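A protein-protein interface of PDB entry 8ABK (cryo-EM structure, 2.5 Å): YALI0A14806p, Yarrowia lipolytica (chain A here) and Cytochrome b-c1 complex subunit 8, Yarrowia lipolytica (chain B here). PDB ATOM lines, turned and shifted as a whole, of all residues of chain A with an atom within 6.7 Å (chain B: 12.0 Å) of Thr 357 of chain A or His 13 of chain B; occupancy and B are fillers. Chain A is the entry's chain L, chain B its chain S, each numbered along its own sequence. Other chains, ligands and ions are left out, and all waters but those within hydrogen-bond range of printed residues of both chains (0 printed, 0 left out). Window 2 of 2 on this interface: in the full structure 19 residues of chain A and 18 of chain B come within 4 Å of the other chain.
The backbone NH (N) of Gly 12 of chain B sits at hydrogen-bond distance from the side-chain carboxylate (OE2) of Glu 457 of chain A (2.9 Å). The side-chain carboxylate (OE2) of Glu 457 of chain A lies within hydrogen-bond range of the backbone NH (N) of His 13 of chain B, at 2.9 Å. OE2 of Glu 457 of chain A lies within hydrogen-bond range of N of Met 14 of chain B, 2.6 Å away. The side-chain carboxylate of Glu 457 of chain A sits close to the backbone carbonyl oxygen of Trp 10 of chain B.
The backbone NH of Gly 9 of chain B sits at hydrogen-bond distance from the backbone carbonyl oxygen of Met 14 of chain B, 2.9 Å away.
Among the printed residues, merely in contact across the chains: Thr 357 of chain A with His 13 of chain B (3.6 Å), Glu 457 of chain A with Trp 11 of chain B (3.7 Å), Thr 356 of chain A with Gly 12 of chain B (3.8 Å) and Gly 458 of chain A with Gly 12 of chain B (3.97 Å).
Thr 357 of chain A touches just one residue of chain B: His 13 (3.6 Å). His 13 of chain B touches just these residues of chain A: Thr 357 and Glu 457. No residue of chain B comes within 4 Å of Asn 355 of chain A. Gln 358 of chain A touches none of the printed residues of chain B. Ile 359 of chain A touches none of the printed residues of chain B. No residue of chain B comes within 4 Å of Asp 360 of chain A. Of the printed residues of chain B, Glu 457 of chain A touches Trp 10, Trp 11, Gly 12, His 13 and Met 14. Of chain B, only Gly 12 comes within 4 Å of Gly 458 of chain A. Printed residues of chain A within 4 Å of Trp 10 of chain B: Glu 457 (3.4 Å). Printed residues of chain A within 4 Å of Gly 12 of chain B: Thr 356 (3.8 Å), Glu 457 (2.9 Å) and Gly 458 (3.97 Å). Of the printed residues of chain A, Met 14 of chain B touches Glu 457. Gly 15 of chain B touches none of the printed residues of chain A. The nearest residue of chain A that does not touch His 13 of chain B is Thr 356 of chain A (6.0 Å). The nearest printed residue of chain A that does not touch Trp 10 of chain B is Thr 357 of chain A (6.3 Å).
Hydrophobic or aromatic side chains of chain B within 4 Å of the printed part of chain A: Trp 11, His 13 and Met 14. Among the printed residues, 8 pairs touch across the chains. Among the printed residues, no Asp or Glu carboxylate lies within 4 Å of a Lys or Arg side-chain nitrogen of the other chain.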
ATOM      1  N   GLU A 354      24.781  -7.070  25.211  1.00  0.00           N
ATOM      2  CA  GLU A 354      25.074  -5.670  24.934  1.00  0.00           C
ATOM      3  C   GLU A 354      23.788  -4.943  24.562  1.00  0.00           C
ATOM      4  O   GLU A 354      23.778  -3.739  24.338  1.00  0.00           O
ATOM      5  CB  GLU A 354      25.972  -5.552  23.705  1.00  0.00           C
ATOM      6  CG  GLU A 354      27.410  -5.995  23.926  1.00  0.00           C
ATOM      7  CD  GLU A 354      28.188  -6.476  22.703  1.00  0.00           C
ATOM      8  OE1 GLU A 354      29.401  -6.783  22.849  1.00  0.00           O
ATOM      9  OE2 GLU A 354      27.586  -6.569  21.602  1.00  0.00           O
ATOM     10  N   ASN A 355      22.697  -5.686  24.450  1.00  0.00           N
ATOM     11  CA  ASN A 355      21.464  -5.105  23.971  1.00  0.00           C
ATOM     12  C   ASN A 355      20.764  -4.488  25.173  1.00  0.00           C
ATOM     13  O   ASN A 355      19.880  -5.095  25.761  1.00  0.00           O
ATOM     14  CB  ASN A 355      20.639  -6.180  23.267  1.00  0.00           C
ATOM     15  CG  ASN A 355      19.398  -5.678  22.558  1.00  0.00           C
ATOM     16  OD1 ASN A 355      18.963  -4.544  22.754  1.00  0.00           O
ATOM     17  ND2 ASN A 355      18.809  -6.534  21.734  1.00  0.00           N
ATOM     18  N   THR A 356      21.130  -3.265  25.525  1.00  0.00           N
ATOM     19  CA  THR A 356      20.742  -2.847  26.857  1.00  0.00           C
ATOM     20  C   THR A 356      19.308  -2.335  26.912  1.00  0.00           C
ATOM     21  O   THR A 356      18.775  -2.151  27.997  1.00  0.00           O
ATOM     22  CB  THR A 356      21.748  -1.863  27.437  1.00  0.00           C
ATOM     23  OG1 THR A 356      21.761  -0.790  26.498  1.00  0.00           O
ATOM     24  CG2 THR A 356      23.106  -2.499  27.629  1.00  0.00           C
ATOM     25  N   THR A 357      18.674  -2.139  25.758  1.00  0.00           N
ATOM     26  CA  THR A 357      17.269  -1.778  25.805  1.00  0.00           C
ATOM     27  C   THR A 357      16.371  -2.998  25.675  1.00  0.00           C
ATOM     28  O   THR A 357      15.153  -2.858  25.674  1.00  0.00           O
ATOM     29  CB  THR A 357      16.895  -0.795  24.698  1.00  0.00           C
ATOM     30  OG1 THR A 357      17.310  -1.455  23.504  1.00  0.00           O
ATOM     31  CG2 THR A 357      17.542   0.560  24.883  1.00  0.00           C
ATOM     32  N   GLN A 358      16.942  -4.195  25.546  1.00  0.00           N
ATOM     33  CA  GLN A 358      16.039  -5.326  25.453  1.00  0.00           C
ATOM     34  C   GLN A 358      16.374  -6.386  26.485  1.00  0.00           C
ATOM     35  O   GLN A 358      16.009  -7.543  26.315  1.00  0.00           O
ATOM     36  CB  GLN A 358      16.034  -5.902  24.048  1.00  0.00           C
ATOM     37  CG  GLN A 358      15.309  -5.009  23.067  1.00  0.00           C
ATOM     38  CD  GLN A 358      15.147  -5.812  21.808  1.00  0.00           C
ATOM     39  OE1 GLN A 358      16.039  -5.835  20.960  1.00  0.00           O
ATOM     40  NE2 GLN A 358      14.045  -6.548  21.728  1.00  0.00           N
ATOM     41  N   ILE A 359      17.016  -5.976  27.575  1.00  0.00           N
ATOM     42  CA  ILE A 359      17.293  -6.898  28.663  1.00  0.00           C
ATOM     43  C   ILE A 359      15.977  -7.476  29.181  1.00  0.00           C
ATOM     44  O   ILE A 359      15.900  -8.658  29.525  1.00  0.00           O
ATOM     45  CB  ILE A 359      18.075  -6.159  29.759  1.00  0.00           C
ATOM     46  CG1 ILE A 359      19.532  -5.981  29.343  1.00  0.00           C
ATOM     47  CG2 ILE A 359      17.954  -6.847  31.115  1.00  0.00           C
ATOM     48  CD1 ILE A 359      20.232  -5.008  30.216  1.00  0.00           C
ATOM     49  N   ASP A 360      14.946  -6.626  29.220  1.00  0.00           N
ATOM     50  CA  ASP A 360      13.629  -7.055  29.647  1.00  0.00           C
ATOM     51  C   ASP A 360      13.153  -8.223  28.787  1.00  0.00           C
ATOM     52  O   ASP A 360      12.685  -9.211  29.349  1.00  0.00           O
ATOM     53  CB  ASP A 360      12.634  -5.899  29.710  1.00  0.00           C
ATOM     54  CG  ASP A 360      12.313  -5.255  28.371  1.00  0.00           C
ATOM     55  OD1 ASP A 360      13.191  -5.248  27.470  1.00  0.00           O
ATOM     56  OD2 ASP A 360      11.183  -4.744  28.245  1.00  0.00           O
ATOM     57  N   ASP A 361      13.313  -8.130  27.453  1.00  0.00           N
ATOM     58  CA  ASP A 361      12.906  -9.202  26.554  1.00  0.00           C
ATOM     59  C   ASP A 361      13.729 -10.455  26.807  1.00  0.00           C
ATOM     60  O   ASP A 361      13.183 -11.558  26.874  1.00  0.00           O
ATOM     61  CB  ASP A 361      12.993  -8.810  25.081  1.00  0.00           C
ATOM     62  CG  ASP A 361      11.971  -7.757  24.712  1.00  0.00           C
ATOM     63  OD1 ASP A 361      10.781  -7.953  25.034  1.00  0.00           O
ATOM     64  OD2 ASP A 361      12.381  -6.735  24.137  1.00  0.00           O
ATOM     65  N   GLU A 457      20.135  -0.990  33.857  1.00  0.00           N
ATOM     66  CA  GLU A 457      18.994  -0.109  34.043  1.00  0.00           C
ATOM     67  C   GLU A 457      17.701  -0.783  33.576  1.00  0.00           C
ATOM     68  O   GLU A 457      16.678  -0.659  34.242  1.00  0.00           O
ATOM     69  CB  GLU A 457      19.188   1.223  33.321  1.00  0.00           C
ATOM     70  CG  GLU A 457      18.028   2.176  33.549  1.00  0.00           C
ATOM     71  CD  GLU A 457      18.126   3.455  32.747  1.00  0.00           C
ATOM     72  OE1 GLU A 457      18.881   4.362  33.159  1.00  0.00           O
ATOM     73  OE2 GLU A 457      17.460   3.533  31.704  1.00  0.00           O
ATOM     74  N   GLY A 458      17.757  -1.498  32.445  1.00  0.00           N
ATOM     75  CA  GLY A 458      16.586  -2.132  31.867  1.00  0.00           C
ATOM     76  C   GLY A 458      16.213  -3.452  32.542  1.00  0.00           C
ATOM     77  O   GLY A 458      15.287  -4.133  32.109  1.00  0.00           O
ATOM     78  N   TYR B   7      13.054  15.114  28.760  1.00  0.00           N
ATOM     79  CA  TYR B   7      13.691  14.978  30.139  1.00  0.00           C
ATOM     80  C   TYR B   7      13.511  13.607  30.784  1.00  0.00           C
ATOM     81  O   TYR B   7      14.007  13.361  31.885  1.00  0.00           O
ATOM     82  CB  TYR B   7      13.193  16.042  31.111  1.00  0.00           C
ATOM     83  CG  TYR B   7      13.773  17.380  30.767  1.00  0.00           C
ATOM     84  CD1 TYR B   7      15.137  17.610  30.866  1.00  0.00           C
ATOM     85  CD2 TYR B   7      12.969  18.391  30.258  1.00  0.00           C
ATOM     86  CE1 TYR B   7      15.684  18.829  30.499  1.00  0.00           C
ATOM     87  CE2 TYR B   7      13.502  19.616  29.889  1.00  0.00           C
ATOM     88  CZ  TYR B   7      14.863  19.836  30.011  1.00  0.00           C
ATOM     89  OH  TYR B   7      15.393  21.039  29.650  1.00  0.00           O
ATOM     90  N   MET B   8      12.775  12.718  30.133  1.00  0.00           N
ATOM     91  CA  MET B   8      12.799  11.355  30.608  1.00  0.00           C
ATOM     92  C   MET B   8      12.963  10.468  29.388  1.00  0.00           C
ATOM     93  O   MET B   8      12.354  10.745  28.363  1.00  0.00           O
ATOM     94  CB  MET B   8      11.501  11.030  31.342  1.00  0.00           C
ATOM     95  CG  MET B   8      11.414   9.576  31.750  1.00  0.00           C
ATOM     96  SD  MET B   8       9.873   9.156  32.591  1.00  0.00           S
ATOM     97  CE  MET B   8       8.758   8.982  31.196  1.00  0.00           C
ATOM     98  N   GLY B   9      13.789   9.421  29.489  1.00  0.00           N
ATOM     99  CA  GLY B   9      13.914   8.520  28.367  1.00  0.00           C
ATOM    100  C   GLY B   9      13.016   7.319  28.593  1.00  0.00           C
ATOM    101  O   GLY B   9      11.823   7.464  28.841  1.00  0.00           O
ATOM    102  N   TRP B  10      13.613   6.136  28.505  1.00  0.00           N
ATOM    103  CA  TRP B  10      12.872   4.906  28.716  1.00  0.00           C
ATOM    104  C   TRP B  10      13.820   3.874  29.306  1.00  0.00           C
ATOM    105  O   TRP B  10      15.006   4.155  29.431  1.00  0.00           O
ATOM    106  CB  TRP B  10      12.268   4.426  27.393  1.00  0.00           C
ATOM    107  CG  TRP B  10      11.058   3.577  27.622  1.00  0.00           C
ATOM    108  CD1 TRP B  10      10.950   2.223  27.482  1.00  0.00           C
ATOM    109  CD2 TRP B  10       9.786   4.031  28.112  1.00  0.00           C
ATOM    110  NE1 TRP B  10       9.687   1.809  27.819  1.00  0.00           N
ATOM    111  CE2 TRP B  10       8.950   2.895  28.212  1.00  0.00           C
ATOM    112  CE3 TRP B  10       9.277   5.293  28.460  1.00  0.00           C
ATOM    113  CZ2 TRP B  10       7.622   2.988  28.633  1.00  0.00           C
ATOM    114  CZ3 TRP B  10       7.958   5.384  28.860  1.00  0.00           C
ATOM    115  CH2 TRP B  10       7.147   4.246  28.947  1.00  0.00           C
ATOM    116  N   TRP B  11      13.325   2.689  29.659  1.00  0.00           N
ATOM    117  CA  TRP B  11      14.198   1.684  30.247  1.00  0.00           C
ATOM    118  C   TRP B  11      15.421   1.424  29.375  1.00  0.00           C
ATOM    119  O   TRP B  11      15.296   1.205  28.174  1.00  0.00           O
ATOM    120  CB  TRP B  11      13.407   0.404  30.404  1.00  0.00           C
ATOM    121  CG  TRP B  11      12.228   0.571  31.298  1.00  0.00           C
ATOM    122  CD1 TRP B  11      10.914   0.602  30.930  1.00  0.00           C
ATOM    123  CD2 TRP B  11      12.260   0.704  32.731  1.00  0.00           C
ATOM    124  NE1 TRP B  11      10.124   0.732  32.042  1.00  0.00           N
ATOM    125  CE2 TRP B  11      10.918   0.801  33.160  1.00  0.00           C
ATOM    126  CE3 TRP B  11      13.285   0.738  33.691  1.00  0.00           C
ATOM    127  CZ2 TRP B  11      10.580   0.945  34.510  1.00  0.00           C
ATOM    128  CZ3 TRP B  11      12.949   0.880  35.025  1.00  0.00           C
ATOM    129  CH2 TRP B  11      11.612   0.987  35.426  1.00  0.00           C
ATOM    130  N   GLY B  12      16.603   1.413  30.000  1.00  0.00           N
ATOM    131  CA  GLY B  12      17.836   1.280  29.249  1.00  0.00           C
ATOM    132  C   GLY B  12      18.498   2.627  28.964  1.00  0.00           C
ATOM    133  O   GLY B  12      19.718   2.677  28.834  1.00  0.00           O
ATOM    134  N   HIS B  13      17.720   3.710  28.869  1.00  0.00           N
ATOM    135  CA  HIS B  13      18.278   5.021  28.577  1.00  0.00           C
ATOM    136  C   HIS B  13      17.392   6.054  29.254  1.00  0.00           C
ATOM    137  O   HIS B  13      16.838   6.937  28.607  1.00  0.00           O
ATOM    138  CB  HIS B  13      18.426   5.232  27.055  1.00  0.00           C
ATOM    139  CG  HIS B  13      17.152   5.057  26.293  1.00  0.00           C
ATOM    140  ND1 HIS B  13      16.633   3.812  26.011  1.00  0.00           N
ATOM    141  CD2 HIS B  13      16.273   5.960  25.791  1.00  0.00           C
ATOM    142  CE1 HIS B  13      15.497   3.949  25.355  1.00  0.00           C
ATOM    143  NE2 HIS B  13      15.247   5.263  25.214  1.00  0.00           N
ATOM    144  N   MET B  14      17.231   5.911  30.566  1.00  0.00           N
ATOM    145  CA  MET B  14      16.262   6.727  31.273  1.00  0.00           C
ATOM    146  C   MET B  14      16.697   8.194  31.328  1.00  0.00           C
ATOM    147  O   MET B  14      15.848   9.070  31.440  1.00  0.00           O
ATOM    148  CB  MET B  14      16.043   6.189  32.689  1.00  0.00           C
ATOM    149  CG  MET B  14      14.789   6.716  33.353  1.00  0.00           C
ATOM    150  SD  MET B  14      13.323   6.049  32.530  1.00  0.00           S
ATOM    151  CE  MET B  14      13.549   4.309  32.898  1.00  0.00           C
ATOM    152  N   GLY B  15      18.001   8.472  31.223  1.00  0.00           N
ATOM    153  CA  GLY B  15      18.479   9.846  31.299  1.00  0.00           C
ATOM    154  C   GLY B  15      19.201  10.153  32.608  1.00  0.00           C
ATOM    155  O   GLY B  15      19.514  11.310  32.883  1.00  0.00           O
ATOM    156  N   SER B  16      19.478   9.108  33.396  1.00  0.00           N
ATOM    157  CA  SER B  16      20.264   9.208  34.613  1.00  0.00           C
ATOM    158  C   SER B  16      21.690   9.572  34.223  1.00  0.00           C
ATOM    159  O   SER B  16      22.174   9.129  33.186  1.00  0.00           O
ATOM    160  CB  SER B  16      20.218   7.894  35.373  1.00  0.00           C
ATOM    161  OG  SER B  16      21.181   7.834  36.420  1.00  0.00           O
ATOM    162  N   PRO B  17      22.413  10.377  35.028  1.00  0.00           N
ATOM    163  CA  PRO B  17      23.865  10.457  34.886  1.00  0.00           C
ATOM    164  C   PRO B  17      24.388   9.036  35.072  1.00  0.00           C
ATOM    165  O   PRO B  17      23.713   8.214  35.683  1.00  0.00           O
ATOM    166  CB  PRO B  17      24.291  11.244  36.123  1.00  0.00           C
ATOM    167  CG  PRO B  17      23.073  12.055  36.479  1.00  0.00           C
ATOM    168  CD  PRO B  17      21.885  11.193  36.130  1.00  0.00           C
ATOM    169  N   PRO B  18      25.585   8.697  34.553  1.00  0.00           N
ATOM    170  CA  PRO B  18      26.129   7.348  34.705  1.00  0.00           C
ATOM    171  C   PRO B  18      26.177   6.924  36.166  1.00  0.00           C
ATOM    172  O   PRO B  18      26.609   7.682  37.029  1.00  0.00           O
ATOM    173  CB  PRO B  18      27.570   7.520  34.233  1.00  0.00           C
ATOM    174  CG  PRO B  18      27.485   8.633  33.231  1.00  0.00           C
ATOM    175  CD  PRO B  18      26.478   9.596  33.809  1.00  0.00           C
ATOM    176  N   GLN B  19      25.721   5.704  36.425  1.00  0.00           N
ATOM    177  CA  GLN B  19      25.750   5.182  37.775  1.00  0.00           C
ATOM    178  C   GLN B  19      26.888   4.186  37.868  1.00  0.00           C
ATOM    179  O   GLN B  19      27.082   3.373  36.972  1.00  0.00           O
ATOM    180  CB  GLN B  19      24.427   4.495  38.087  1.00  0.00           C
ATOM    181  CG  GLN B  19      23.240   5.419  37.903  1.00  0.00           C
ATOM    182  CD  GLN B  19      21.999   4.914  38.593  1.00  0.00           C
ATOM    183  OE1 GLN B  19      22.030   3.945  39.356  1.00  0.00           O
ATOM    184  NE2 GLN B  19      20.882   5.570  38.322  1.00  0.00           N
